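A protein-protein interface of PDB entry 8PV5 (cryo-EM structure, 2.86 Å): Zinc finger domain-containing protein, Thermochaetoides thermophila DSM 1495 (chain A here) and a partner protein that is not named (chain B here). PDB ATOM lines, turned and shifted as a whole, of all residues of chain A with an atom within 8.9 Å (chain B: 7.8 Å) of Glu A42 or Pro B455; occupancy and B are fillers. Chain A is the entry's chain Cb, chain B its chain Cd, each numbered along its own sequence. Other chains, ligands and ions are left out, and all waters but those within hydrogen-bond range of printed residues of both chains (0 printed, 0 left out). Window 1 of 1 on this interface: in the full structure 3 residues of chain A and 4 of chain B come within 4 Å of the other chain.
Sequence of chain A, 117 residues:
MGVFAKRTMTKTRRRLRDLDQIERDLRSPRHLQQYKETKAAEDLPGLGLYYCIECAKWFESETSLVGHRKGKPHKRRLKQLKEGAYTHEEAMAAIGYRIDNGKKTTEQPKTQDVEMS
Among the printed residues, merely in contact across the chains: Pro A45 with Gly B452 (3.2 Å), Asp A43 with Glu B454 (3.6 Å), Glu A42 with Glu B440 (3.8 Å) and Glu A42 with Pro B455 (3.9 Å).
Printed residues of chain B that touch a printed residue of chain A: Glu B440, Gly B452, Glu B454 and Pro B455.
Hydrophobic or aromatic side chains of chain B that line the printed part of chain A: Pro B455.
Of the 12 printed residues of chain A, 3 touch a printed residue of chain B.
Hydrophobic or aromatic side chains of chain A that line the printed part of chain B: Pro A45.
Among the printed residues, no Asp or Glu carboxylate lies within 4 Å of a Lys or Arg side-chain nitrogen of the other chain.
Of chain A, only Glu A42 comes within 4 Å of Pro B455.
No residue of chain B comes within 4 Å of Ala A41.
Of the printed residues of chain A, Gly B452 touches Pro A45.
Of the printed residues of chain A, Glu B454 touches Asp A43 (3.6 Å).
Of the printed residues of chain A, Glu B440 touches Glu A42.
Printed residues of chain B within 4 Å of Asp A43: Glu B454.
Asp B456 touches none of the printed residues of chain A.
Lys B451 touches none of the printed residues of chain A.
The nearest residue of chain B that does not touch Glu A42 is Glu B454 (5.1 Å).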
ATOM      1  N   LYS A  36     -22.142 -17.084  -9.239  1.00  0.00           N
ATOM      2  CA  LYS A  36     -23.143 -17.825  -8.474  1.00  0.00           C
ATOM      3  C   LYS A  36     -23.435 -19.189  -9.087  1.00  0.00           C
ATOM      4  O   LYS A  36     -23.607 -20.168  -8.351  1.00  0.00           O
ATOM      5  CB  LYS A  36     -24.436 -17.019  -8.355  1.00  0.00           C
ATOM      6  CG  LYS A  36     -24.320 -15.759  -7.519  1.00  0.00           C
ATOM      7  CD  LYS A  36     -24.134 -16.086  -6.051  1.00  0.00           C
ATOM      8  CE  LYS A  36     -24.082 -14.823  -5.216  1.00  0.00           C
ATOM      9  NZ  LYS A  36     -25.405 -14.144  -5.171  1.00  0.00           N
ATOM     10  N   LYS A  39     -20.923 -22.118  -8.153  1.00  0.00           N
ATOM     11  CA  LYS A  39     -21.078 -22.879  -6.922  1.00  0.00           C
ATOM     12  C   LYS A  39     -22.438 -23.565  -6.882  1.00  0.00           C
ATOM     13  O   LYS A  39     -23.298 -23.347  -7.741  1.00  0.00           O
ATOM     14  CB  LYS A  39     -20.926 -21.979  -5.687  1.00  0.00           C
ATOM     15  CG  LYS A  39     -19.738 -21.037  -5.732  1.00  0.00           C
ATOM     16  CD  LYS A  39     -18.444 -21.768  -5.426  1.00  0.00           C
ATOM     17  CE  LYS A  39     -17.296 -20.792  -5.240  1.00  0.00           C
ATOM     18  NZ  LYS A  39     -16.069 -21.471  -4.742  1.00  0.00           N
ATOM     19  N   ALA A  40     -22.621 -24.401  -5.862  1.00  0.00           N
ATOM     20  CA  ALA A  40     -23.871 -25.111  -5.620  1.00  0.00           C
ATOM     21  C   ALA A  40     -24.589 -24.445  -4.453  1.00  0.00           C
ATOM     22  O   ALA A  40     -23.985 -24.225  -3.400  1.00  0.00           O
ATOM     23  CB  ALA A  40     -23.617 -26.589  -5.325  1.00  0.00           C
ATOM     24  N   ALA A  41     -25.877 -24.144  -4.643  1.00  0.00           N
ATOM     25  CA  ALA A  41     -26.597 -23.296  -3.696  1.00  0.00           C
ATOM     26  C   ALA A  41     -26.869 -24.012  -2.378  1.00  0.00           C
ATOM     27  O   ALA A  41     -26.894 -23.377  -1.316  1.00  0.00           O
ATOM     28  CB  ALA A  41     -27.905 -22.813  -4.319  1.00  0.00           C
ATOM     29  N   GLU A  42     -27.090 -25.326  -2.421  1.00  0.00           N
ATOM     30  CA  GLU A  42     -27.461 -26.050  -1.209  1.00  0.00           C
ATOM     31  C   GLU A  42     -26.289 -26.231  -0.250  1.00  0.00           C
ATOM     32  O   GLU A  42     -26.513 -26.521   0.930  1.00  0.00           O
ATOM     33  CB  GLU A  42     -28.059 -27.411  -1.567  1.00  0.00           C
ATOM     34  CG  GLU A  42     -27.094 -28.368  -2.248  1.00  0.00           C
ATOM     35  CD  GLU A  42     -27.147 -28.280  -3.761  1.00  0.00           C
ATOM     36  OE1 GLU A  42     -27.738 -27.313  -4.285  1.00  0.00           O
ATOM     37  OE2 GLU A  42     -26.601 -29.185  -4.426  1.00  0.00           O
ATOM     38  N   ASP A  43     -25.057 -26.066  -0.721  1.00  0.00           N
ATOM     39  CA  ASP A  43     -23.879 -26.162   0.130  1.00  0.00           C
ATOM     40  C   ASP A  43     -23.445 -24.816   0.695  1.00  0.00           C
ATOM     41  O   ASP A  43     -22.426 -24.751   1.390  1.00  0.00           O
ATOM     42  CB  ASP A  43     -22.719 -26.792  -0.646  1.00  0.00           C
ATOM     43  CG  ASP A  43     -23.096 -28.113  -1.280  1.00  0.00           C
ATOM     44  OD1 ASP A  43     -22.382 -28.556  -2.203  1.00  0.00           O
ATOM     45  OD2 ASP A  43     -24.107 -28.708  -0.853  1.00  0.00           O
ATOM     46  N   LEU A  44     -24.183 -23.757   0.418  1.00  0.00           N
ATOM     47  CA  LEU A  44     -23.888 -22.395   0.820  1.00  0.00           C
ATOM     48  C   LEU A  44     -24.467 -22.099   2.200  1.00  0.00           C
ATOM     49  O   LEU A  44     -25.480 -22.686   2.594  1.00  0.00           O
ATOM     50  CB  LEU A  44     -24.464 -21.408  -0.199  1.00  0.00           C
ATOM     51  CG  LEU A  44     -23.890 -21.506  -1.615  1.00  0.00           C
ATOM     52  CD1 LEU A  44     -24.269 -20.296  -2.432  1.00  0.00           C
ATOM     53  CD2 LEU A  44     -22.375 -21.666  -1.592  1.00  0.00           C
ATOM     54  N   PRO A  45     -23.830 -21.209   2.961  1.00  0.00           N
ATOM     55  CA  PRO A  45     -24.411 -20.782   4.239  1.00  0.00           C
ATOM     56  C   PRO A  45     -25.703 -20.007   4.023  1.00  0.00           C
ATOM     57  O   PRO A  45     -25.752 -19.048   3.249  1.00  0.00           O
ATOM     58  CB  PRO A  45     -23.321 -19.892   4.848  1.00  0.00           C
ATOM     59  CG  PRO A  45     -22.069 -20.254   4.139  1.00  0.00           C
ATOM     60  CD  PRO A  45     -22.459 -20.706   2.773  1.00  0.00           C
ATOM     61  N   GLY A  46     -26.754 -20.426   4.725  1.00  0.00           N
ATOM     62  CA  GLY A  46     -28.046 -19.785   4.580  1.00  0.00           C
ATOM     63  C   GLY A  46     -28.688 -19.977   3.227  1.00  0.00           C
ATOM     64  O   GLY A  46     -29.461 -19.117   2.793  1.00  0.00           O
ATOM     65  N   LEU A  47     -28.366 -21.079   2.542  1.00  0.00           N
ATOM     66  CA  LEU A  47     -28.858 -21.421   1.204  1.00  0.00           C
ATOM     67  C   LEU A  47     -28.510 -20.359   0.164  1.00  0.00           C
ATOM     68  O   LEU A  47     -29.229 -20.198  -0.827  1.00  0.00           O
ATOM     69  CB  LEU A  47     -30.372 -21.688   1.198  1.00  0.00           C
ATOM     70  CG  LEU A  47     -30.926 -23.062   1.598  1.00  0.00           C
ATOM     71  CD1 LEU A  47     -30.461 -24.134   0.620  1.00  0.00           C
ATOM     72  CD2 LEU A  47     -30.602 -23.454   3.037  1.00  0.00           C
ATOM     73  N   GLY A  48     -27.416 -19.627   0.372  1.00  0.00           N
ATOM     74  CA  GLY A  48     -26.986 -18.601  -0.554  1.00  0.00           C
ATOM     75  C   GLY A  48     -27.789 -17.322  -0.521  1.00  0.00           C
ATOM     76  O   GLY A  48     -27.572 -16.454  -1.376  1.00  0.00           O
ATOM     77  N   LEU A  49     -28.705 -17.169   0.436  1.00  0.00           N
ATOM     78  CA  LEU A  49     -29.572 -15.999   0.473  1.00  0.00           C
ATOM     79  C   LEU A  49     -28.870 -14.757   1.003  1.00  0.00           C
ATOM     80  O   LEU A  49     -29.359 -13.645   0.775  1.00  0.00           O
ATOM     81  CB  LEU A  49     -30.806 -16.294   1.325  1.00  0.00           C
ATOM     82  CG  LEU A  49     -31.759 -17.359   0.780  1.00  0.00           C
ATOM     83  CD1 LEU A  49     -32.863 -17.655   1.782  1.00  0.00           C
ATOM     84  CD2 LEU A  49     -32.343 -16.925  -0.554  1.00  0.00           C
ATOM     85  N   ILE B 436     -33.152 -36.312   0.139  1.00  0.00           N
ATOM     86  CA  ILE B 436     -32.030 -35.409   0.388  1.00  0.00           C
ATOM     87  C   ILE B 436     -32.515 -34.142   1.087  1.00  0.00           C
ATOM     88  O   ILE B 436     -31.819 -33.584   1.945  1.00  0.00           O
ATOM     89  CB  ILE B 436     -31.262 -35.115  -0.918  1.00  0.00           C
ATOM     90  CG1 ILE B 436     -29.931 -34.421  -0.614  1.00  0.00           C
ATOM     91  CG2 ILE B 436     -32.090 -34.324  -1.929  1.00  0.00           C
ATOM     92  CD1 ILE B 436     -28.954 -35.291   0.140  1.00  0.00           C
ATOM     93  N   GLU B 437     -33.738 -33.701   0.773  1.00  0.00           N
ATOM     94  CA  GLU B 437     -34.331 -32.584   1.500  1.00  0.00           C
ATOM     95  C   GLU B 437     -34.589 -32.956   2.951  1.00  0.00           C
ATOM     96  O   GLU B 437     -34.345 -32.151   3.855  1.00  0.00           O
ATOM     97  CB  GLU B 437     -35.626 -32.136   0.821  1.00  0.00           C
ATOM     98  CG  GLU B 437     -36.390 -31.058   1.570  1.00  0.00           C
ATOM     99  CD  GLU B 437     -36.040 -29.662   1.097  1.00  0.00           C
ATOM    100  OE1 GLU B 437     -35.343 -29.540   0.069  1.00  0.00           O
ATOM    101  OE2 GLU B 437     -36.459 -28.688   1.756  1.00  0.00           O
ATOM    102  N   LEU B 439     -32.922 -35.200   4.723  1.00  0.00           N
ATOM    103  CA  LEU B 439     -31.622 -35.257   5.387  1.00  0.00           C
ATOM    104  C   LEU B 439     -31.084 -33.861   5.680  1.00  0.00           C
ATOM    105  O   LEU B 439     -30.540 -33.618   6.763  1.00  0.00           O
ATOM    106  CB  LEU B 439     -30.621 -36.043   4.538  1.00  0.00           C
ATOM    107  CG  LEU B 439     -30.881 -37.526   4.256  1.00  0.00           C
ATOM    108  CD1 LEU B 439     -29.791 -38.088   3.356  1.00  0.00           C
ATOM    109  CD2 LEU B 439     -31.015 -38.351   5.524  1.00  0.00           C
ATOM    110  N   GLU B 440     -31.239 -32.928   4.733  1.00  0.00           N
ATOM    111  CA  GLU B 440     -30.760 -31.563   4.943  1.00  0.00           C
ATOM    112  C   GLU B 440     -31.532 -30.862   6.056  1.00  0.00           C
ATOM    113  O   GLU B 440     -30.939 -30.171   6.894  1.00  0.00           O
ATOM    114  CB  GLU B 440     -30.854 -30.764   3.643  1.00  0.00           C
ATOM    115  CG  GLU B 440     -29.790 -31.111   2.617  1.00  0.00           C
ATOM    116  CD  GLU B 440     -29.960 -30.337   1.326  1.00  0.00           C
ATOM    117  OE1 GLU B 440     -30.949 -29.584   1.209  1.00  0.00           O
ATOM    118  OE2 GLU B 440     -29.103 -30.478   0.428  1.00  0.00           O
ATOM    119  N   MET B 441     -32.859 -31.025   6.076  1.00  0.00           N
ATOM    120  CA  MET B 441     -33.672 -30.413   7.123  1.00  0.00           C
ATOM    121  C   MET B 441     -33.333 -30.986   8.493  1.00  0.00           C
ATOM    122  O   MET B 441     -33.237 -30.247   9.479  1.00  0.00           O
ATOM    123  CB  MET B 441     -35.159 -30.592   6.816  1.00  0.00           C
ATOM    124  CG  MET B 441     -35.645 -29.835   5.590  1.00  0.00           C
ATOM    125  SD  MET B 441     -37.381 -30.147   5.215  1.00  0.00           S
ATOM    126  CE  MET B 441     -38.185 -29.292   6.565  1.00  0.00           C
ATOM    127  N   LEU B 442     -33.116 -32.303   8.570  1.00  0.00           N
ATOM    128  CA  LEU B 442     -32.795 -32.903   9.860  1.00  0.00           C
ATOM    129  C   LEU B 442     -31.390 -32.506  10.306  1.00  0.00           C
ATOM    130  O   LEU B 442     -31.137 -32.341  11.505  1.00  0.00           O
ATOM    131  CB  LEU B 442     -32.950 -34.424   9.779  1.00  0.00           C
ATOM    132  CG  LEU B 442     -32.862 -35.313  11.029  1.00  0.00           C
ATOM    133  CD1 LEU B 442     -33.674 -36.563  10.754  1.00  0.00           C
ATOM    134  CD2 LEU B 442     -31.459 -35.699  11.486  1.00  0.00           C
ATOM    135  N   ALA B 443     -30.465 -32.341   9.353  1.00  0.00           N
ATOM    136  CA  ALA B 443     -29.123 -31.866   9.683  1.00  0.00           C
ATOM    137  C   ALA B 443     -29.152 -30.440  10.215  1.00  0.00           C
ATOM    138  O   ALA B 443     -28.456 -30.118  11.184  1.00  0.00           O
ATOM    139  CB  ALA B 443     -28.221 -31.948   8.454  1.00  0.00           C
ATOM    140  N   ARG B 444     -29.946 -29.570   9.587  1.00  0.00           N
ATOM    141  CA  ARG B 444     -30.059 -28.198  10.069  1.00  0.00           C
ATOM    142  C   ARG B 444     -30.784 -28.140  11.408  1.00  0.00           C
ATOM    143  O   ARG B 444     -30.536 -27.238  12.216  1.00  0.00           O
ATOM    144  CB  ARG B 444     -30.772 -27.336   9.031  1.00  0.00           C
ATOM    145  CG  ARG B 444     -29.868 -26.843   7.915  1.00  0.00           C
ATOM    146  CD  ARG B 444     -30.553 -25.771   7.086  1.00  0.00           C
ATOM    147  NE  ARG B 444     -31.762 -26.272   6.444  1.00  0.00           N
ATOM    148  CZ  ARG B 444     -31.780 -26.971   5.316  1.00  0.00           C
ATOM    149  NH1 ARG B 444     -30.665 -27.267   4.669  1.00  0.00           N
ATOM    150  NH2 ARG B 444     -32.947 -27.380   4.826  1.00  0.00           N
ATOM    151  N   GLY B 447     -28.037 -29.721  14.029  1.00  0.00           N
ATOM    152  CA  GLY B 447     -26.705 -29.153  14.098  1.00  0.00           C
ATOM    153  C   GLY B 447     -25.621 -29.989  13.460  1.00  0.00           C
ATOM    154  O   GLY B 447     -24.445 -29.807  13.779  1.00  0.00           O
ATOM    155  N   ARG B 448     -25.984 -30.907  12.564  1.00  0.00           N
ATOM    156  CA  ARG B 448     -25.004 -31.715  11.838  1.00  0.00           C
ATOM    157  C   ARG B 448     -24.456 -30.873  10.690  1.00  0.00           C
ATOM    158  O   ARG B 448     -24.881 -30.973   9.536  1.00  0.00           O
ATOM    159  CB  ARG B 448     -25.634 -33.009  11.339  1.00  0.00           C
ATOM    160  CG  ARG B 448     -26.164 -33.928  12.434  1.00  0.00           C
ATOM    161  CD  ARG B 448     -25.061 -34.385  13.367  1.00  0.00           C
ATOM    162  NE  ARG B 448     -25.026 -33.594  14.590  1.00  0.00           N
ATOM    163  CZ  ARG B 448     -23.951 -33.433  15.346  1.00  0.00           C
ATOM    164  NH1 ARG B 448     -22.793 -33.985  15.028  1.00  0.00           N
ATOM    165  NH2 ARG B 448     -24.037 -32.689  16.443  1.00  0.00           N
ATOM    166  N   LEU B 449     -23.491 -30.021  11.022  1.00  0.00           N
ATOM    167  CA  LEU B 449     -22.949 -29.046  10.090  1.00  0.00           C
ATOM    168  C   LEU B 449     -21.448 -29.235   9.928  1.00  0.00           C
ATOM    169  O   LEU B 449     -20.728 -29.502  10.894  1.00  0.00           O
ATOM    170  CB  LEU B 449     -23.238 -27.615  10.554  1.00  0.00           C
ATOM    171  CG  LEU B 449     -24.684 -27.305  10.934  1.00  0.00           C
ATOM    172  CD1 LEU B 449     -24.779 -25.958  11.630  1.00  0.00           C
ATOM    173  CD2 LEU B 449     -25.574 -27.340   9.703  1.00  0.00           C
ATOM    174  N   LEU B 450     -20.987 -29.099   8.690  1.00  0.00           N
ATOM    175  CA  LEU B 450     -19.567 -29.114   8.381  1.00  0.00           C
ATOM    176  C   LEU B 450     -19.042 -27.679   8.391  1.00  0.00           C
ATOM    177  O   LEU B 450     -19.715 -26.755   8.855  1.00  0.00           O
ATOM    178  CB  LEU B 450     -19.327 -29.809   7.043  1.00  0.00           C
ATOM    179  CG  LEU B 450     -19.794 -31.262   6.953  1.00  0.00           C
ATOM    180  CD1 LEU B 450     -19.627 -31.793   5.539  1.00  0.00           C
ATOM    181  CD2 LEU B 450     -19.044 -32.129   7.949  1.00  0.00           C
ATOM    182  N   LYS B 451     -17.821 -27.482   7.895  1.00  0.00           N
ATOM    183  CA  LYS B 451     -17.273 -26.138   7.764  1.00  0.00           C
ATOM    184  C   LYS B 451     -18.076 -25.337   6.747  1.00  0.00           C
ATOM    185  O   LYS B 451     -18.360 -25.816   5.646  1.00  0.00           O
ATOM    186  CB  LYS B 451     -15.803 -26.199   7.350  1.00  0.00           C
ATOM    187  CG  LYS B 451     -14.920 -26.988   8.300  1.00  0.00           C
ATOM    188  CD  LYS B 451     -14.985 -26.419   9.707  1.00  0.00           C
ATOM    189  CE  LYS B 451     -14.186 -27.261  10.684  1.00  0.00           C
ATOM    190  NZ  LYS B 451     -14.313 -26.753  12.077  1.00  0.00           N
ATOM    191  N   GLY B 452     -18.438 -24.116   7.122  1.00  0.00           N
ATOM    192  CA  GLY B 452     -19.318 -23.304   6.312  1.00  0.00           C
ATOM    193  C   GLY B 452     -20.794 -23.525   6.554  1.00  0.00           C
ATOM    194  O   GLY B 452     -21.613 -22.962   5.820  1.00  0.00           O
ATOM    195  N   GLY B 453     -21.162 -24.331   7.545  1.00  0.00           N
ATOM    196  CA  GLY B 453     -22.557 -24.531   7.874  1.00  0.00           C
ATOM    197  C   GLY B 453     -23.336 -25.401   6.915  1.00  0.00           C
ATOM    198  O   GLY B 453     -24.568 -25.436   7.002  1.00  0.00           O
ATOM    199  N   GLU B 454     -22.667 -26.093   6.000  1.00  0.00           N
ATOM    200  CA  GLU B 454     -23.367 -26.977   5.076  1.00  0.00           C
ATOM    201  C   GLU B 454     -23.865 -28.213   5.820  1.00  0.00           C
ATOM    202  O   GLU B 454     -23.237 -28.634   6.798  1.00  0.00           O
ATOM    203  CB  GLU B 454     -22.453 -27.368   3.912  1.00  0.00           C
ATOM    204  CG  GLU B 454     -21.247 -28.208   4.290  1.00  0.00           C
ATOM    205  CD  GLU B 454     -20.350 -28.505   3.106  1.00  0.00           C
ATOM    206  OE1 GLU B 454     -20.660 -28.035   1.992  1.00  0.00           O
ATOM    207  OE2 GLU B 454     -19.335 -29.211   3.288  1.00  0.00           O
ATOM    208  N   PRO B 455     -25.000 -28.790   5.424  1.00  0.00           N
ATOM    209  CA  PRO B 455     -25.523 -29.963   6.136  1.00  0.00           C
ATOM    210  C   PRO B 455     -24.637 -31.189   5.956  1.00  0.00           C
ATOM    211  O   PRO B 455     -24.019 -31.384   4.907  1.00  0.00           O
ATOM    212  CB  PRO B 455     -26.907 -30.167   5.508  1.00  0.00           C
ATOM    213  CG  PRO B 455     -26.827 -29.494   4.182  1.00  0.00           C
ATOM    214  CD  PRO B 455     -25.928 -28.320   4.382  1.00  0.00           C
ATOM    215  N   ASP B 456     -24.580 -32.020   7.000  1.00  0.00           N
ATOM    216  CA  ASP B 456     -23.815 -33.269   6.975  1.00  0.00           C
ATOM    217  C   ASP B 456     -24.782 -34.420   6.713  1.00  0.00           C
ATOM    218  O   ASP B 456     -25.158 -35.189   7.606  1.00  0.00           O
ATOM    219  CB  ASP B 456     -23.047 -33.453   8.277  1.00  0.00           C
ATOM    220  CG  ASP B 456     -22.004 -34.550   8.190  1.00  0.00           C
ATOM    221  OD1 ASP B 456     -21.757 -35.054   7.075  1.00  0.00           O
ATOM    222  OD2 ASP B 456     -21.432 -34.908   9.241  1.00  0.00           O
ATOM    223  N   VAL B 457     -25.181 -34.538   5.442  1.00  0.00           N
ATOM    224  CA  VAL B 457     -26.176 -35.532   5.053  1.00  0.00           C
ATOM    225  C   VAL B 457     -25.621 -36.946   5.192  1.00  0.00           C
ATOM    226  O   VAL B 457     -26.376 -37.893   5.416  1.00  0.00           O
ATOM    227  CB  VAL B 457     -26.687 -35.248   3.628  1.00  0.00           C
ATOM    228  CG1 VAL B 457     -27.357 -33.887   3.576  1.00  0.00           C
ATOM    229  CG2 VAL B 457     -25.552 -35.312   2.619  1.00  0.00           C
ATOM    230  N   ASP B 458     -24.296 -37.104   5.105  1.00  0.00           N
ATOM    231  CA  ASP B 458     -23.681 -38.417   5.289  1.00  0.00           C
ATOM    232  C   ASP B 458     -23.851 -38.909   6.726  1.00  0.00           C
ATOM    233  O   ASP B 458     -24.313 -40.036   6.959  1.00  0.00           O
ATOM    234  CB  ASP B 458     -22.201 -38.335   4.895  1.00  0.00           C
ATOM    235  CG  ASP B 458     -21.460 -39.657   5.041  1.00  0.00           C
ATOM    236  OD1 ASP B 458     -21.136 -40.062   6.178  1.00  0.00           O
ATOM    237  OD2 ASP B 458     -21.181 -40.288   4.001  1.00  0.00           O
ATOM    238  N   GLY B 459     -23.498 -38.067   7.699  1.00  0.00           N
ATOM    239  CA  GLY B 459     -23.667 -38.447   9.092  1.00  0.00           C
ATOM    240  C   GLY B 459     -25.125 -38.583   9.482  1.00  0.00           C
ATOM    241  O   GLY B 459     -25.490 -39.452  10.280  1.00  0.00           O
ATOM    242  N   VAL B 460     -25.981 -37.728   8.915  1.00  0.00           N
ATOM    243  CA  VAL B 460     -27.416 -37.829   9.175  1.00  0.00           C
ATOM    244  C   VAL B 460     -27.975 -39.137   8.623  1.00  0.00           C
ATOM    245  O   VAL B 460     -28.795 -39.801   9.272  1.00  0.00           O
ATOM    246  CB  VAL B 460     -28.138 -36.595   8.608  1.00  0.00           C
ATOM    247  CG1 VAL B 460     -29.629 -36.809   8.546  1.00  0.00           C
ATOM    248  CG2 VAL B 460     -27.846 -35.409   9.481  1.00  0.00           C
